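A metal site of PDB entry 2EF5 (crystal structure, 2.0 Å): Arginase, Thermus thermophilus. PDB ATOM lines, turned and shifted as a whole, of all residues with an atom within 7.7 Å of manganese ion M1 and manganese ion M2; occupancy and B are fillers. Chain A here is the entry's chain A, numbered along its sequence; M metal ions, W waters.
The backbone NH (N) of His 96 sits at hydrogen-bond distance from the side-chain carboxylate (OE2) of Glu 262 (2.9 Å).
N of Asp 217 sits at hydrogen-bond distance from O of Val 117, 2.9 Å away.
OD2 of Asp 122 lies close to NE1 of Trp 116 (2.9 Å).
The side-chain carboxylate (OD2) of Asp 118 sits close to the indole nitrogen (NE1) of Trp 116.
OD1 of Asp 118 lies close to N of His 120 (2.7 Å).
A ring nitrogen (NE2) of His 96 sits close to the side-chain hydroxyl (OG) of Ser 99, 3.4 Å away.
OD1 of Asp 219 is in hydrogen-bond range of N of Ala 119, 3.0 Å away.
OG of Ser 215 is in hydrogen-bond range of NE2 of His 96.
Four residues have an atom within 4 Å of manganese ion M1: His 96, Asp 118, Asp 122 and Asp 217.
Manganese ion M2 is bound by OD2 of Asp 219 (2.2 Å), OD1 of Asp 118 (2.2 Å) and OD2 of Asp 217 (2.5 Å).
Manganese ion M2 has three donor atoms within binding distance.
Slightly farther from manganese ion M2 lies ND1 of His 120 (2.8 Å).
The side-chain carboxylate (OD2) of Asp 118 is bound to manganese ion M1 (2.1 Å).
Manganese ion M1 is bound by ND1 of His 96.
Manganese ion M1 is bound by the side-chain carboxylate (OD2) of Asp 122 (2.2 Å).
The side-chain carboxylate (OD2) of Asp 217 binds manganese ion M1 (2.4 Å).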
ATOM      1  N   ASP A  95     -23.911 -19.230 -21.311  1.00  0.00           N
ATOM      2  CA  ASP A  95     -23.723 -20.575 -20.771  1.00  0.00           C
ATOM      3  C   ASP A  95     -24.993 -21.390 -20.652  1.00  0.00           C
ATOM      4  O   ASP A  95     -26.039 -20.879 -20.246  1.00  0.00           O
ATOM      5  CB  ASP A  95     -23.101 -20.526 -19.381  1.00  0.00           C
ATOM      6  CG  ASP A  95     -21.773 -19.812 -19.352  1.00  0.00           C
ATOM      7  OD1 ASP A  95     -20.992 -19.982 -20.313  1.00  0.00           O
ATOM      8  OD2 ASP A  95     -21.501 -19.108 -18.360  1.00  0.00           O
ATOM      9  N   HIS A  96     -24.886 -22.684 -20.948  1.00  0.00           N
ATOM     10  CA  HIS A  96     -26.026 -23.580 -20.832  1.00  0.00           C
ATOM     11  C   HIS A  96     -26.383 -23.763 -19.352  1.00  0.00           C
ATOM     12  O   HIS A  96     -27.420 -24.321 -19.024  1.00  0.00           O
ATOM     13  CB  HIS A  96     -25.681 -24.938 -21.441  1.00  0.00           C
ATOM     14  CG  HIS A  96     -26.877 -25.656 -21.992  1.00  0.00           C
ATOM     15  ND1 HIS A  96     -26.768 -26.656 -22.939  1.00  0.00           N
ATOM     16  CD2 HIS A  96     -28.192 -25.472 -21.769  1.00  0.00           C
ATOM     17  CE1 HIS A  96     -27.985 -27.041 -23.286  1.00  0.00           C
ATOM     18  NE2 HIS A  96     -28.863 -26.348 -22.603  1.00  0.00           N
ATOM     19  N   SER A  97     -25.510 -23.274 -18.476  1.00  0.00           N
ATOM     20  CA  SER A  97     -25.722 -23.355 -17.032  1.00  0.00           C
ATOM     21  C   SER A  97     -27.051 -22.700 -16.664  1.00  0.00           C
ATOM     22  O   SER A  97     -27.689 -23.093 -15.696  1.00  0.00           O
ATOM     23  CB  SER A  97     -24.602 -22.639 -16.272  1.00  0.00           C
ATOM     24  OG  SER A  97     -23.349 -23.237 -16.505  1.00  0.00           O
ATOM     25  N   SER A  99     -29.791 -23.074 -17.824  1.00  0.00           N
ATOM     26  CA  SER A  99     -30.900 -24.016 -17.870  1.00  0.00           C
ATOM     27  C   SER A  99     -31.304 -24.556 -16.501  1.00  0.00           C
ATOM     28  O   SER A  99     -32.425 -25.022 -16.338  1.00  0.00           O
ATOM     29  CB  SER A  99     -30.583 -25.179 -18.817  1.00  0.00           C
ATOM     30  OG  SER A  99     -30.618 -24.738 -20.176  1.00  0.00           O
ATOM     31  N   TRP A 116     -33.175 -32.257 -24.537  1.00  0.00           N
ATOM     32  CA  TRP A 116     -31.876 -31.576 -24.559  1.00  0.00           C
ATOM     33  C   TRP A 116     -31.210 -31.827 -25.899  1.00  0.00           C
ATOM     34  O   TRP A 116     -30.733 -32.937 -26.178  1.00  0.00           O
ATOM     35  CB  TRP A 116     -31.038 -32.117 -23.393  1.00  0.00           C
ATOM     36  CG  TRP A 116     -29.923 -31.235 -22.893  1.00  0.00           C
ATOM     37  CD1 TRP A 116     -28.617 -31.236 -23.319  1.00  0.00           C
ATOM     38  CD2 TRP A 116     -30.001 -30.275 -21.819  1.00  0.00           C
ATOM     39  NE1 TRP A 116     -27.876 -30.341 -22.566  1.00  0.00           N
ATOM     40  CE2 TRP A 116     -28.679 -29.757 -21.654  1.00  0.00           C
ATOM     41  CE3 TRP A 116     -31.034 -29.839 -20.992  1.00  0.00           C
ATOM     42  CZ2 TRP A 116     -28.403 -28.784 -20.667  1.00  0.00           C
ATOM     43  CZ3 TRP A 116     -30.743 -28.859 -20.019  1.00  0.00           C
ATOM     44  CH2 TRP A 116     -29.427 -28.357 -19.861  1.00  0.00           C
ATOM     45  N   VAL A 117     -31.212 -30.809 -26.745  1.00  0.00           N
ATOM     46  CA  VAL A 117     -30.657 -30.909 -28.106  1.00  0.00           C
ATOM     47  C   VAL A 117     -29.297 -30.246 -28.020  1.00  0.00           C
ATOM     48  O   VAL A 117     -29.170 -29.023 -28.031  1.00  0.00           O
ATOM     49  CB  VAL A 117     -31.605 -30.203 -29.105  1.00  0.00           C
ATOM     50  CG1 VAL A 117     -31.267 -30.598 -30.522  1.00  0.00           C
ATOM     51  CG2 VAL A 117     -33.047 -30.561 -28.761  1.00  0.00           C
ATOM     52  N   ASP A 118     -28.280 -31.103 -27.978  1.00  0.00           N
ATOM     53  CA  ASP A 118     -26.922 -30.635 -27.732  1.00  0.00           C
ATOM     54  C   ASP A 118     -25.893 -31.624 -28.264  1.00  0.00           C
ATOM     55  O   ASP A 118     -26.168 -32.817 -28.351  1.00  0.00           O
ATOM     56  CB  ASP A 118     -26.801 -30.579 -26.215  1.00  0.00           C
ATOM     57  CG  ASP A 118     -25.737 -29.651 -25.741  1.00  0.00           C
ATOM     58  OD1 ASP A 118     -24.593 -29.698 -26.245  1.00  0.00           O
ATOM     59  OD2 ASP A 118     -26.069 -28.894 -24.807  1.00  0.00           O
ATOM     60  N   ALA A 119     -24.701 -31.124 -28.580  1.00  0.00           N
ATOM     61  CA  ALA A 119     -23.630 -32.000 -29.040  1.00  0.00           C
ATOM     62  C   ALA A 119     -23.051 -32.672 -27.795  1.00  0.00           C
ATOM     63  O   ALA A 119     -22.364 -33.691 -27.894  1.00  0.00           O
ATOM     64  CB  ALA A 119     -22.547 -31.205 -29.752  1.00  0.00           C
ATOM     65  N   HIS A 120     -23.330 -32.094 -26.632  1.00  0.00           N
ATOM     66  CA  HIS A 120     -22.844 -32.640 -25.367  1.00  0.00           C
ATOM     67  C   HIS A 120     -24.030 -33.022 -24.478  1.00  0.00           C
ATOM     68  O   HIS A 120     -25.161 -32.603 -24.740  1.00  0.00           O
ATOM     69  CB  HIS A 120     -21.968 -31.622 -24.630  1.00  0.00           C
ATOM     70  CG  HIS A 120     -20.855 -31.091 -25.467  1.00  0.00           C
ATOM     71  ND1 HIS A 120     -20.987 -29.975 -26.269  1.00  0.00           N
ATOM     72  CD2 HIS A 120     -19.595 -31.552 -25.666  1.00  0.00           C
ATOM     73  CE1 HIS A 120     -19.853 -29.771 -26.927  1.00  0.00           C
ATOM     74  NE2 HIS A 120     -18.996 -30.717 -26.588  1.00  0.00           N
ATOM     75  N   ALA A 121     -23.762 -33.782 -23.428  1.00  0.00           N
ATOM     76  CA  ALA A 121     -24.808 -34.227 -22.512  1.00  0.00           C
ATOM     77  C   ALA A 121     -24.939 -33.342 -21.285  1.00  0.00           C
ATOM     78  O   ALA A 121     -25.977 -33.372 -20.612  1.00  0.00           O
ATOM     79  CB  ALA A 121     -24.539 -35.669 -22.080  1.00  0.00           C
ATOM     80  N   ASP A 122     -23.915 -32.556 -20.992  1.00  0.00           N
ATOM     81  CA  ASP A 122     -23.921 -31.665 -19.828  1.00  0.00           C
ATOM     82  C   ASP A 122     -24.393 -32.431 -18.606  1.00  0.00           C
ATOM     83  O   ASP A 122     -25.142 -31.908 -17.779  1.00  0.00           O
ATOM     84  CB  ASP A 122     -24.845 -30.471 -20.061  1.00  0.00           C
ATOM     85  CG  ASP A 122     -24.406 -29.595 -21.208  1.00  0.00           C
ATOM     86  OD1 ASP A 122     -23.181 -29.381 -21.375  1.00  0.00           O
ATOM     87  OD2 ASP A 122     -25.280 -29.118 -21.964  1.00  0.00           O
ATOM     88  N   HIS A 135     -21.111 -25.157 -16.631  1.00  0.00           N
ATOM     89  CA  HIS A 135     -21.948 -25.269 -17.814  1.00  0.00           C
ATOM     90  C   HIS A 135     -21.863 -26.652 -18.452  1.00  0.00           C
ATOM     91  O   HIS A 135     -22.472 -26.917 -19.489  1.00  0.00           O
ATOM     92  CB  HIS A 135     -21.624 -24.160 -18.823  1.00  0.00           C
ATOM     93  CG  HIS A 135     -20.166 -24.036 -19.172  1.00  0.00           C
ATOM     94  ND1 HIS A 135     -19.480 -25.006 -19.865  1.00  0.00           N
ATOM     95  CD2 HIS A 135     -19.293 -23.020 -18.967  1.00  0.00           C
ATOM     96  CE1 HIS A 135     -18.243 -24.589 -20.078  1.00  0.00           C
ATOM     97  NE2 HIS A 135     -18.105 -23.390 -19.547  1.00  0.00           N
ATOM     98  N   GLY A 136     -21.117 -27.546 -17.809  1.00  0.00           N
ATOM     99  CA  GLY A 136     -20.989 -28.903 -18.297  1.00  0.00           C
ATOM    100  C   GLY A 136     -21.703 -29.845 -17.339  1.00  0.00           C
ATOM    101  O   GLY A 136     -21.550 -31.058 -17.413  1.00  0.00           O
ATOM    102  N   PRO A 138     -25.247 -28.724 -15.962  1.00  0.00           N
ATOM    103  CA  PRO A 138     -26.666 -28.389 -15.752  1.00  0.00           C
ATOM    104  C   PRO A 138     -27.725 -29.488 -15.842  1.00  0.00           C
ATOM    105  O   PRO A 138     -28.644 -29.511 -15.033  1.00  0.00           O
ATOM    106  CB  PRO A 138     -26.909 -27.271 -16.767  1.00  0.00           C
ATOM    107  CG  PRO A 138     -26.006 -27.639 -17.891  1.00  0.00           C
ATOM    108  CD  PRO A 138     -24.735 -28.026 -17.159  1.00  0.00           C
ATOM    109  N   SER A 215     -34.406 -27.532 -24.736  1.00  0.00           N
ATOM    110  CA  SER A 215     -33.201 -26.765 -24.487  1.00  0.00           C
ATOM    111  C   SER A 215     -32.302 -26.962 -25.694  1.00  0.00           C
ATOM    112  O   SER A 215     -31.749 -28.050 -25.893  1.00  0.00           O
ATOM    113  CB  SER A 215     -32.515 -27.245 -23.197  1.00  0.00           C
ATOM    114  OG  SER A 215     -31.579 -26.295 -22.757  1.00  0.00           O
ATOM    115  N   LEU A 216     -32.163 -25.922 -26.494  1.00  0.00           N
ATOM    116  CA  LEU A 216     -31.368 -25.996 -27.713  1.00  0.00           C
ATOM    117  C   LEU A 216     -29.997 -25.334 -27.636  1.00  0.00           C
ATOM    118  O   LEU A 216     -29.883 -24.110 -27.526  1.00  0.00           O
ATOM    119  CB  LEU A 216     -32.184 -25.412 -28.877  1.00  0.00           C
ATOM    120  CG  LEU A 216     -31.564 -25.327 -30.278  1.00  0.00           C
ATOM    121  CD1 LEU A 216     -31.197 -26.720 -30.780  1.00  0.00           C
ATOM    122  CD2 LEU A 216     -32.585 -24.678 -31.229  1.00  0.00           C
ATOM    123  N   ASP A 217     -28.957 -26.153 -27.675  1.00  0.00           N
ATOM    124  CA  ASP A 217     -27.583 -25.679 -27.650  1.00  0.00           C
ATOM    125  C   ASP A 217     -27.172 -25.543 -29.121  1.00  0.00           C
ATOM    126  O   ASP A 217     -27.288 -26.495 -29.876  1.00  0.00           O
ATOM    127  CB  ASP A 217     -26.664 -26.683 -26.951  1.00  0.00           C
ATOM    128  CG  ASP A 217     -25.267 -26.146 -26.749  1.00  0.00           C
ATOM    129  OD1 ASP A 217     -24.711 -25.556 -27.688  1.00  0.00           O
ATOM    130  OD2 ASP A 217     -24.714 -26.311 -25.643  1.00  0.00           O
ATOM    131  N   ALA A 218     -26.710 -24.363 -29.497  1.00  0.00           N
ATOM    132  CA  ALA A 218     -26.312 -24.100 -30.873  1.00  0.00           C
ATOM    133  C   ALA A 218     -25.295 -25.096 -31.407  1.00  0.00           C
ATOM    134  O   ALA A 218     -25.262 -25.365 -32.606  1.00  0.00           O
ATOM    135  CB  ALA A 218     -25.752 -22.686 -31.007  1.00  0.00           C
ATOM    136  N   ASP A 219     -24.465 -25.658 -30.519  1.00  0.00           N
ATOM    137  CA  ASP A 219     -23.451 -26.578 -30.976  1.00  0.00           C
ATOM    138  C   ASP A 219     -23.945 -27.934 -31.458  1.00  0.00           C
ATOM    139  O   ASP A 219     -23.149 -28.752 -31.873  1.00  0.00           O
ATOM    140  CB  ASP A 219     -22.366 -26.777 -29.911  1.00  0.00           C
ATOM    141  CG  ASP A 219     -22.824 -27.617 -28.735  1.00  0.00           C
ATOM    142  OD1 ASP A 219     -23.896 -28.246 -28.793  1.00  0.00           O
ATOM    143  OD2 ASP A 219     -22.079 -27.669 -27.738  1.00  0.00           O
ATOM    144  N   VAL A 220     -25.255 -28.173 -31.402  1.00  0.00           N
ATOM    145  CA  VAL A 220     -25.780 -29.459 -31.877  1.00  0.00           C
ATOM    146  C   VAL A 220     -25.717 -29.452 -33.407  1.00  0.00           C
ATOM    147  O   VAL A 220     -25.634 -30.495 -34.038  1.00  0.00           O
ATOM    148  CB  VAL A 220     -27.251 -29.682 -31.424  1.00  0.00           C
ATOM    149  CG1 VAL A 220     -28.190 -28.761 -32.192  1.00  0.00           C
ATOM    150  CG2 VAL A 220     -27.635 -31.135 -31.629  1.00  0.00           C
ATOM    151  N   VAL A 229     -19.914 -21.116 -31.857  1.00  0.00           N
ATOM    152  CA  VAL A 229     -20.116 -21.879 -30.627  1.00  0.00           C
ATOM    153  C   VAL A 229     -18.783 -22.132 -29.926  1.00  0.00           C
ATOM    154  O   VAL A 229     -17.750 -22.285 -30.576  1.00  0.00           O
ATOM    155  CB  VAL A 229     -20.798 -23.249 -30.905  1.00  0.00           C
ATOM    156  CG1 VAL A 229     -22.123 -23.026 -31.638  1.00  0.00           C
ATOM    157  CG2 VAL A 229     -19.889 -24.135 -31.734  1.00  0.00           C
ATOM    158  N   THR A 231     -17.697 -24.806 -28.057  1.00  0.00           N
ATOM    159  CA  THR A 231     -17.123 -26.132 -28.225  1.00  0.00           C
ATOM    160  C   THR A 231     -17.676 -26.855 -29.445  1.00  0.00           C
ATOM    161  O   THR A 231     -18.502 -27.761 -29.334  1.00  0.00           O
ATOM    162  CB  THR A 231     -17.365 -26.986 -26.962  1.00  0.00           C
ATOM    163  OG1 THR A 231     -17.048 -26.212 -25.799  1.00  0.00           O
ATOM    164  CG2 THR A 231     -16.492 -28.221 -26.979  1.00  0.00           C
ATOM    165  N   VAL A 233     -18.109 -29.379 -32.505  1.00  0.00           N
ATOM    166  CA  VAL A 233     -17.803 -30.786 -32.687  1.00  0.00           C
ATOM    167  C   VAL A 233     -18.323 -31.179 -34.070  1.00  0.00           C
ATOM    168  O   VAL A 233     -19.524 -31.054 -34.345  1.00  0.00           O
ATOM    169  CB  VAL A 233     -18.485 -31.662 -31.615  1.00  0.00           C
ATOM    170  CG1 VAL A 233     -17.995 -33.093 -31.734  1.00  0.00           C
ATOM    171  CG2 VAL A 233     -18.195 -31.099 -30.226  1.00  0.00           C
ATOM    172  N   VAL A 261     -29.339 -21.438 -26.332  1.00  0.00           N
ATOM    173  CA  VAL A 261     -28.067 -21.165 -25.683  1.00  0.00           C
ATOM    174  C   VAL A 261     -26.789 -21.383 -26.473  1.00  0.00           C
ATOM    175  O   VAL A 261     -26.796 -21.902 -27.581  1.00  0.00           O
ATOM    176  CB  VAL A 261     -27.943 -22.026 -24.391  1.00  0.00           C
ATOM    177  CG1 VAL A 261     -29.133 -21.780 -23.466  1.00  0.00           C
ATOM    178  CG2 VAL A 261     -27.873 -23.505 -24.772  1.00  0.00           C
ATOM    179  N   GLU A 262     -25.691 -20.968 -25.840  1.00  0.00           N
ATOM    180  CA  GLU A 262     -24.331 -21.108 -26.358  1.00  0.00           C
ATOM    181  C   GLU A 262     -23.976 -20.402 -27.671  1.00  0.00           C
ATOM    182  O   GLU A 262     -22.996 -20.748 -28.320  1.00  0.00           O
ATOM    183  CB  GLU A 262     -24.000 -22.600 -26.460  1.00  0.00           C
ATOM    184  CG  GLU A 262     -23.988 -23.333 -25.104  1.00  0.00           C
ATOM    185  CD  GLU A 262     -22.742 -23.040 -24.267  1.00  0.00           C
ATOM    186  OE1 GLU A 262     -21.640 -22.965 -24.841  1.00  0.00           O
ATOM    187  OE2 GLU A 262     -22.856 -22.878 -23.037  1.00  0.00           O
HETATM  188 MN    MN M   1     -24.906 -27.640 -23.594  1.00  0.00          MN
HETATM  189 MN    MN M   2     -23.049 -28.161 -25.816  1.00  0.00          MN
HETATM  190  O   HOH W   1     -21.338 -26.535 -23.615  1.00  0.00           O
